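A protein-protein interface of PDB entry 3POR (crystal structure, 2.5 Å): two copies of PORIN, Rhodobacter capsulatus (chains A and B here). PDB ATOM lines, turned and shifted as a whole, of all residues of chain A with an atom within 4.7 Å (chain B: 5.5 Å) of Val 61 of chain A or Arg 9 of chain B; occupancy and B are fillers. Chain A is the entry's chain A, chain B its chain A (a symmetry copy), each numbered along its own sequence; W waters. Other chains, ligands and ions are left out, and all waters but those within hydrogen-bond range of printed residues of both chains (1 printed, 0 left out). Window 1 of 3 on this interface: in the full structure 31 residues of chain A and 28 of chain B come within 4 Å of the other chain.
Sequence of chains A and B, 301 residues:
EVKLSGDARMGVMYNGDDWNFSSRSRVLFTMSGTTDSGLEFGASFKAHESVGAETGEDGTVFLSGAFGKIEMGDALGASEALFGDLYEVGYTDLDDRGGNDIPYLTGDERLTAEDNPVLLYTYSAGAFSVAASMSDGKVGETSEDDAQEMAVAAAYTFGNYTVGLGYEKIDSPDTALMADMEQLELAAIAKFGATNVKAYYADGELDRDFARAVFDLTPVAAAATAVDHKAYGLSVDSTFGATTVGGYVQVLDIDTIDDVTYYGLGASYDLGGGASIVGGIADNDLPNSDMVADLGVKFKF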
ATOM      1  N   GLY A  42      -3.800 -23.535  -0.770  1.00  0.00           N
ATOM      2  CA  GLY A  42      -3.273 -24.116  -1.999  1.00  0.00           C
ATOM      3  C   GLY A  42      -2.034 -24.915  -1.731  1.00  0.00           C
ATOM      4  O   GLY A  42      -1.653 -25.068  -0.572  1.00  0.00           O
ATOM      5  N   ALA A  43      -1.411 -25.354  -2.798  1.00  0.00           N
ATOM      6  CA  ALA A  43      -0.299 -26.238  -2.713  1.00  0.00           C
ATOM      7  C   ALA A  43       0.371 -26.185  -4.032  1.00  0.00           C
ATOM      8  O   ALA A  43      -0.346 -25.951  -4.988  1.00  0.00           O
ATOM      9  CB  ALA A  43      -0.764 -27.646  -2.507  1.00  0.00           C
ATOM     10  N   GLY A  59       8.026 -28.671  -2.391  1.00  0.00           N
ATOM     11  CA  GLY A  59       6.725 -28.125  -2.616  1.00  0.00           C
ATOM     12  C   GLY A  59       6.271 -27.357  -1.398  1.00  0.00           C
ATOM     13  O   GLY A  59       6.980 -27.376  -0.406  1.00  0.00           O
ATOM     14  N   THR A  60       5.186 -26.598  -1.404  1.00  0.00           N
ATOM     15  CA  THR A  60       4.746 -25.895  -0.205  1.00  0.00           C
ATOM     16  C   THR A  60       3.266 -26.024  -0.078  1.00  0.00           C
ATOM     17  O   THR A  60       2.697 -26.230  -1.140  1.00  0.00           O
ATOM     18  CB  THR A  60       4.980 -24.466  -0.262  1.00  0.00           C
ATOM     19  OG1 THR A  60       4.357 -24.067  -1.468  1.00  0.00           O
ATOM     20  CG2 THR A  60       6.443 -24.078  -0.287  1.00  0.00           C
ATOM     21  N   VAL A  61       2.630 -25.969   1.079  1.00  0.00           N
ATOM     22  CA  VAL A  61       1.188 -25.980   1.235  1.00  0.00           C
ATOM     23  C   VAL A  61       0.913 -24.646   1.942  1.00  0.00           C
ATOM     24  O   VAL A  61       1.810 -24.139   2.643  1.00  0.00           O
ATOM     25  CB  VAL A  61       0.768 -27.167   2.099  1.00  0.00           C
ATOM     26  CG1 VAL A  61      -0.725 -27.183   2.368  1.00  0.00           C
ATOM     27  CG2 VAL A  61       1.103 -28.398   1.353  1.00  0.00           C
ATOM     28  N   PHE A  62      -0.235 -23.971   1.788  1.00  0.00           N
ATOM     29  CA  PHE A  62      -0.491 -22.735   2.537  1.00  0.00           C
ATOM     30  C   PHE A  62      -1.955 -22.503   2.799  1.00  0.00           C
ATOM     31  O   PHE A  62      -2.778 -23.132   2.147  1.00  0.00           O
ATOM     32  CB  PHE A  62       0.056 -21.528   1.800  1.00  0.00           C
ATOM     33  CG  PHE A  62      -0.777 -21.110   0.646  1.00  0.00           C
ATOM     34  CD1 PHE A  62      -1.823 -20.231   0.836  1.00  0.00           C
ATOM     35  CD2 PHE A  62      -0.474 -21.630  -0.578  1.00  0.00           C
ATOM     36  CE1 PHE A  62      -2.616 -19.851  -0.222  1.00  0.00           C
ATOM     37  CE2 PHE A  62      -1.260 -21.252  -1.643  1.00  0.00           C
ATOM     38  CZ  PHE A  62      -2.324 -20.373  -1.466  1.00  0.00           C
ATOM     39  N   ILE A  70       0.214 -18.756   6.178  1.00  0.00           N
ATOM     40  CA  ILE A  70       1.116 -19.669   6.807  1.00  0.00           C
ATOM     41  C   ILE A  70       1.534 -20.589   5.701  1.00  0.00           C
ATOM     42  O   ILE A  70       0.656 -21.145   5.045  1.00  0.00           O
ATOM     43  CB  ILE A  70       0.408 -20.437   7.771  1.00  0.00           C
ATOM     44  CG1 ILE A  70      -0.087 -19.575   8.853  1.00  0.00           C
ATOM     45  CG2 ILE A  70       1.362 -21.380   8.425  1.00  0.00           C
ATOM     46  CD1 ILE A  70      -1.303 -20.428   9.363  1.00  0.00           C
ATOM     47  N   GLU A  71       2.805 -20.853   5.472  1.00  0.00           N
ATOM     48  CA  GLU A  71       3.173 -21.795   4.431  1.00  0.00           C
ATOM     49  C   GLU A  71       4.056 -22.892   5.043  1.00  0.00           C
ATOM     50  O   GLU A  71       4.845 -22.617   5.952  1.00  0.00           O
ATOM     51  CB  GLU A  71       3.845 -20.954   3.436  1.00  0.00           C
ATOM     52  CG  GLU A  71       4.379 -21.693   2.294  1.00  0.00           C
ATOM     53  CD  GLU A  71       4.684 -20.719   1.197  1.00  0.00           C
ATOM     54  OE1 GLU A  71       5.506 -19.841   1.403  1.00  0.00           O
ATOM     55  OE2 GLU A  71       4.088 -20.842   0.121  1.00  0.00           O
ATOM     56  N   MET A  72       3.980 -24.144   4.622  1.00  0.00           N
ATOM     57  CA  MET A  72       4.747 -25.196   5.215  1.00  0.00           C
ATOM     58  C   MET A  72       5.316 -26.040   4.111  1.00  0.00           C
ATOM     59  O   MET A  72       4.644 -26.135   3.097  1.00  0.00           O
ATOM     60  CB  MET A  72       3.864 -26.001   6.096  1.00  0.00           C
ATOM     61  CG  MET A  72       4.615 -27.078   6.835  1.00  0.00           C
ATOM     62  SD  MET A  72       3.681 -27.740   8.222  1.00  0.00           S
ATOM     63  CE  MET A  72       3.456 -26.252   9.152  1.00  0.00           C
ATOM     64  N   ASP B   7      -4.456 -33.106  -3.578  1.00  0.00           N
ATOM     65  CA  ASP B   7      -4.786 -32.869  -2.169  1.00  0.00           C
ATOM     66  C   ASP B   7      -3.525 -32.344  -1.498  1.00  0.00           C
ATOM     67  O   ASP B   7      -2.469 -32.255  -2.164  1.00  0.00           O
ATOM     68  CB  ASP B   7      -5.279 -34.148  -1.412  1.00  0.00           C
ATOM     69  CG  ASP B   7      -4.490 -35.451  -1.544  1.00  0.00           C
ATOM     70  OD1 ASP B   7      -3.271 -35.429  -1.428  1.00  0.00           O
ATOM     71  OD2 ASP B   7      -5.079 -36.501  -1.748  1.00  0.00           O
ATOM     72  N   ALA B   8      -3.656 -31.909  -0.253  1.00  0.00           N
ATOM     73  CA  ALA B   8      -2.546 -31.383   0.476  1.00  0.00           C
ATOM     74  C   ALA B   8      -2.960 -31.372   1.923  1.00  0.00           C
ATOM     75  O   ALA B   8      -4.160 -31.529   2.145  1.00  0.00           O
ATOM     76  CB  ALA B   8      -2.250 -30.013  -0.012  1.00  0.00           C
ATOM     77  N   ARG B   9      -2.093 -31.335   2.960  1.00  0.00           N
ATOM     78  CA  ARG B   9      -2.504 -31.186   4.349  1.00  0.00           C
ATOM     79  C   ARG B   9      -1.388 -30.497   5.071  1.00  0.00           C
ATOM     80  O   ARG B   9      -0.326 -30.386   4.505  1.00  0.00           O
ATOM     81  CB  ARG B   9      -2.734 -32.488   4.961  1.00  0.00           C
ATOM     82  CG  ARG B   9      -1.498 -33.307   4.994  1.00  0.00           C
ATOM     83  CD  ARG B   9      -1.942 -34.667   5.268  1.00  0.00           C
ATOM     84  NE  ARG B   9      -0.768 -35.486   5.368  1.00  0.00           N
ATOM     85  CZ  ARG B   9      -0.860 -36.831   5.362  1.00  0.00           C
ATOM     86  NH1 ARG B   9      -2.030 -37.488   5.304  1.00  0.00           N
ATOM     87  NH2 ARG B   9       0.247 -37.549   5.452  1.00  0.00           N
ATOM     88  N   MET B  10      -1.503 -29.911   6.235  1.00  0.00           N
ATOM     89  CA  MET B  10      -0.384 -29.375   6.972  1.00  0.00           C
ATOM     90  C   MET B  10      -0.812 -29.295   8.396  1.00  0.00           C
ATOM     91  O   MET B  10      -2.022 -29.254   8.597  1.00  0.00           O
ATOM     92  CB  MET B  10       0.027 -28.001   6.555  1.00  0.00           C
ATOM     93  CG  MET B  10      -0.886 -26.855   6.242  1.00  0.00           C
ATOM     94  SD  MET B  10       0.042 -25.316   5.980  1.00  0.00           S
ATOM     95  CE  MET B  10      -1.374 -24.437   6.533  1.00  0.00           C
ATOM     96  N   GLY B  11       0.035 -29.367   9.408  1.00  0.00           N
ATOM     97  CA  GLY B  11      -0.368 -29.280  10.803  1.00  0.00           C
ATOM     98  C   GLY B  11       0.809 -29.787  11.620  1.00  0.00           C
ATOM     99  O   GLY B  11       1.974 -29.785  11.183  1.00  0.00           O
ATOM    100  N   SER B  22       4.031 -31.598   9.968  1.00  0.00           N
ATOM    101  CA  SER B  22       3.897 -32.671   9.019  1.00  0.00           C
ATOM    102  C   SER B  22       3.094 -32.055   7.890  1.00  0.00           C
ATOM    103  O   SER B  22       2.099 -31.388   8.240  1.00  0.00           O
ATOM    104  CB  SER B  22       3.143 -33.760   9.652  1.00  0.00           C
ATOM    105  OG  SER B  22       3.115 -34.870   8.755  1.00  0.00           O
ATOM    106  N   SER B  23       3.483 -32.210   6.598  1.00  0.00           N
ATOM    107  CA  SER B  23       2.707 -31.769   5.449  1.00  0.00           C
ATOM    108  C   SER B  23       2.995 -32.525   4.151  1.00  0.00           C
ATOM    109  O   SER B  23       3.916 -33.334   4.095  1.00  0.00           O
ATOM    110  CB  SER B  23       2.936 -30.356   5.173  1.00  0.00           C
ATOM    111  OG  SER B  23       4.280 -30.243   4.811  1.00  0.00           O
ATOM    112  N   ARG B  24       2.156 -32.366   3.139  1.00  0.00           N
ATOM    113  CA  ARG B  24       2.332 -33.037   1.892  1.00  0.00           C
ATOM    114  C   ARG B  24       1.399 -32.472   0.893  1.00  0.00           C
ATOM    115  O   ARG B  24       0.445 -31.851   1.325  1.00  0.00           O
ATOM    116  CB  ARG B  24       2.021 -34.495   1.942  1.00  0.00           C
ATOM    117  CG  ARG B  24       0.686 -34.925   2.262  1.00  0.00           C
ATOM    118  CD  ARG B  24       0.790 -36.336   1.757  1.00  0.00           C
ATOM    119  NE  ARG B  24      -0.541 -36.875   1.805  1.00  0.00           N
ATOM    120  CZ  ARG B  24      -0.816 -38.148   1.959  1.00  0.00           C
ATOM    121  NH1 ARG B  24       0.157 -39.032   2.075  1.00  0.00           N
ATOM    122  NH2 ARG B  24      -2.095 -38.547   1.995  1.00  0.00           N
ATOM    123  N   SER B  25       1.694 -32.692  -0.372  1.00  0.00           N
ATOM    124  CA  SER B  25       0.756 -32.439  -1.412  1.00  0.00           C
ATOM    125  C   SER B  25       0.914 -33.572  -2.410  1.00  0.00           C
ATOM    126  O   SER B  25       2.025 -34.104  -2.547  1.00  0.00           O
ATOM    127  CB  SER B  25       1.027 -31.094  -2.038  1.00  0.00           C
ATOM    128  OG  SER B  25       2.374 -30.912  -2.380  1.00  0.00           O
ATOM    129  N   TYR B  91      -5.534 -36.018  10.898  1.00  0.00           N
ATOM    130  CA  TYR B  91      -5.286 -35.432   9.588  1.00  0.00           C
ATOM    131  C   TYR B  91      -4.197 -36.138   8.846  1.00  0.00           C
ATOM    132  O   TYR B  91      -4.116 -35.960   7.659  1.00  0.00           O
ATOM    133  CB  TYR B  91      -4.923 -33.935   9.692  1.00  0.00           C
ATOM    134  CG  TYR B  91      -3.480 -33.543   9.717  1.00  0.00           C
ATOM    135  CD1 TYR B  91      -2.738 -33.385   8.599  1.00  0.00           C
ATOM    136  CD2 TYR B  91      -2.934 -33.273  10.924  1.00  0.00           C
ATOM    137  CE1 TYR B  91      -1.455 -32.928   8.733  1.00  0.00           C
ATOM    138  CE2 TYR B  91      -1.658 -32.824  11.062  1.00  0.00           C
ATOM    139  CZ  TYR B  91      -0.926 -32.649   9.959  1.00  0.00           C
ATOM    140  OH  TYR B  91       0.345 -32.126  10.125  1.00  0.00           O
ATOM    141  N   THR B  92      -3.246 -36.769   9.507  1.00  0.00           N
ATOM    142  CA  THR B  92      -2.218 -37.541   8.850  1.00  0.00           C
ATOM    143  C   THR B  92      -2.709 -38.996   8.819  1.00  0.00           C
ATOM    144  O   THR B  92      -1.938 -39.767   8.306  1.00  0.00           O
ATOM    145  CB  THR B  92      -0.841 -37.437   9.610  1.00  0.00           C
ATOM    146  OG1 THR B  92      -1.141 -37.651  10.951  1.00  0.00           O
ATOM    147  CG2 THR B  92      -0.201 -36.093   9.732  1.00  0.00           C
ATOM    148  N   ASP B  93      -3.907 -39.485   9.188  1.00  0.00           N
ATOM    149  CA  ASP B  93      -4.306 -40.894   9.203  1.00  0.00           C
ATOM    150  C   ASP B  93      -3.408 -41.498  10.245  1.00  0.00           C
ATOM    151  O   ASP B  93      -2.281 -41.909   9.928  1.00  0.00           O
ATOM    152  CB  ASP B  93      -4.090 -41.600   7.834  1.00  0.00           C
ATOM    153  CG  ASP B  93      -4.750 -42.972   7.680  1.00  0.00           C
ATOM    154  OD1 ASP B  93      -5.245 -43.443   8.707  1.00  0.00           O
ATOM    155  OD2 ASP B  93      -4.795 -43.573   6.580  1.00  0.00           O
ATOM    156  N   VAL B 297      -4.871 -29.043   8.867  1.00  0.00           N
ATOM    157  CA  VAL B 297      -5.901 -28.799   7.895  1.00  0.00           C
ATOM    158  C   VAL B 297      -5.703 -29.739   6.742  1.00  0.00           C
ATOM    159  O   VAL B 297      -4.572 -30.088   6.466  1.00  0.00           O
ATOM    160  CB  VAL B 297      -5.850 -27.360   7.411  1.00  0.00           C
ATOM    161  CG1 VAL B 297      -6.333 -26.451   8.477  1.00  0.00           C
ATOM    162  CG2 VAL B 297      -4.450 -26.912   7.161  1.00  0.00           C
ATOM    163  N   LYS B 298      -6.714 -30.139   6.010  1.00  0.00           N
ATOM    164  CA  LYS B 298      -6.627 -31.109   4.951  1.00  0.00           C
ATOM    165  C   LYS B 298      -7.344 -30.381   3.790  1.00  0.00           C
ATOM    166  O   LYS B 298      -8.265 -29.610   4.069  1.00  0.00           O
ATOM    167  CB  LYS B 298      -7.314 -32.253   5.627  1.00  0.00           C
ATOM    168  CG  LYS B 298      -6.956 -33.639   5.208  1.00  0.00           C
ATOM    169  CD  LYS B 298      -7.634 -34.589   6.107  1.00  0.00           C
ATOM    170  CE  LYS B 298      -8.069 -35.842   5.314  1.00  0.00           C
ATOM    171  NZ  LYS B 298      -8.679 -36.886   6.145  1.00  0.00           N
ATOM    172  N   PHE B 299      -7.001 -30.490   2.488  1.00  0.00           N
ATOM    173  CA  PHE B 299      -7.421 -29.650   1.369  1.00  0.00           C
ATOM    174  C   PHE B 299      -7.620 -30.565   0.225  1.00  0.00           C
ATOM    175  O   PHE B 299      -6.827 -31.459   0.085  1.00  0.00           O
ATOM    176  CB  PHE B 299      -6.375 -28.766   0.921  1.00  0.00           C
ATOM    177  CG  PHE B 299      -5.898 -27.697   1.889  1.00  0.00           C
ATOM    178  CD1 PHE B 299      -6.745 -27.105   2.779  1.00  0.00           C
ATOM    179  CD2 PHE B 299      -4.563 -27.307   1.846  1.00  0.00           C
ATOM    180  CE1 PHE B 299      -6.229 -26.132   3.617  1.00  0.00           C
ATOM    181  CE2 PHE B 299      -4.055 -26.339   2.685  1.00  0.00           C
ATOM    182  CZ  PHE B 299      -4.901 -25.750   3.578  1.00  0.00           C
HETATM  183  O   HOH W   1       4.504 -29.248   2.313  1.00  0.00           O
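Of the 15 printed residues of chain B, 9 touch a printed residue of chain A.
Hydrophobic or aromatic side chains of chain B within 4 Å of the printed part of chain A: Ala 8, Met 10 and Phe 299.
Printed residues of chain A that touch a printed residue of chain B: Ala 43, Val 61, Phe 62 and Met 72.
Among the printed residues, no Asp or Glu carboxylate lies within 4 Å of a Lys or Arg side-chain nitrogen of the other chain.
N of Gly 11 of chain B sits close to OH of Tyr 91 of chain B, 2.9 Å away.
The backbone carbonyl oxygen of Gly 11 of chain B sits at hydrogen-bond distance from the backbone NH of Ser 22 of chain B, 3.0 Å away.
The backbone carbonyl oxygen (O) of Met 72 of chain A lies within hydrogen-bond range of the backbone NH (N) of Val 61 of chain A (2.9 Å).
The guanidinium group of Arg 9 of chain B lies close to the backbone carbonyl oxygen of Tyr 91 of chain B (3.5 Å).
The backbone carbonyl oxygen (O) of Met 10 of chain B sits at hydrogen-bond distance from the backbone NH (N) of Val 297 of chain B (2.9 Å).
The backbone carbonyl oxygen of Ala 8 of chain B is in hydrogen-bond range of the backbone NH of Phe 299 of chain B (3.0 Å).
No position is printed for both chains.
Water W1 bridges OG of Ser 23 of chain B and O of Met 72 of chain A.
Of the printed residues of chain B, Met 72 of chain A touches Met 10 (3.9 Å), Gly 11 (3.98 Å), Ser 22 (3.98 Å) and Ser 23 (3.8 Å).
Of chain A, only Val 61 comes within 4 Å of Arg 9 of chain B.
Printed residues of chain A within 4 Å of Gly 11 of chain B: Met 72 (3.98 Å).
Among the printed residues, merely in contact across the chains: Val 61 of chain A with Phe 299 of chain B, Phe 62 of chain A with Phe 299 of chain B, Val 61 of chain A with Arg 24 of chain B, Ala 43 of chain A with Ala 8 of chain B, Met 72 of chain A with Ser 23 of chain B, Val 61 of chain A with Arg 9 of chain B, Met 72 of chain A with Met 10 of chain B, Val 61 of chain A with Met 10 of chain B, Ala 43 of chain A with Ser 25 of chain B, Val 61 of chain A with Ala 8 of chain B, Met 72 of chain A with Ser 22 of chain B and Met 72 of chain A with Gly 11 of chain B.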
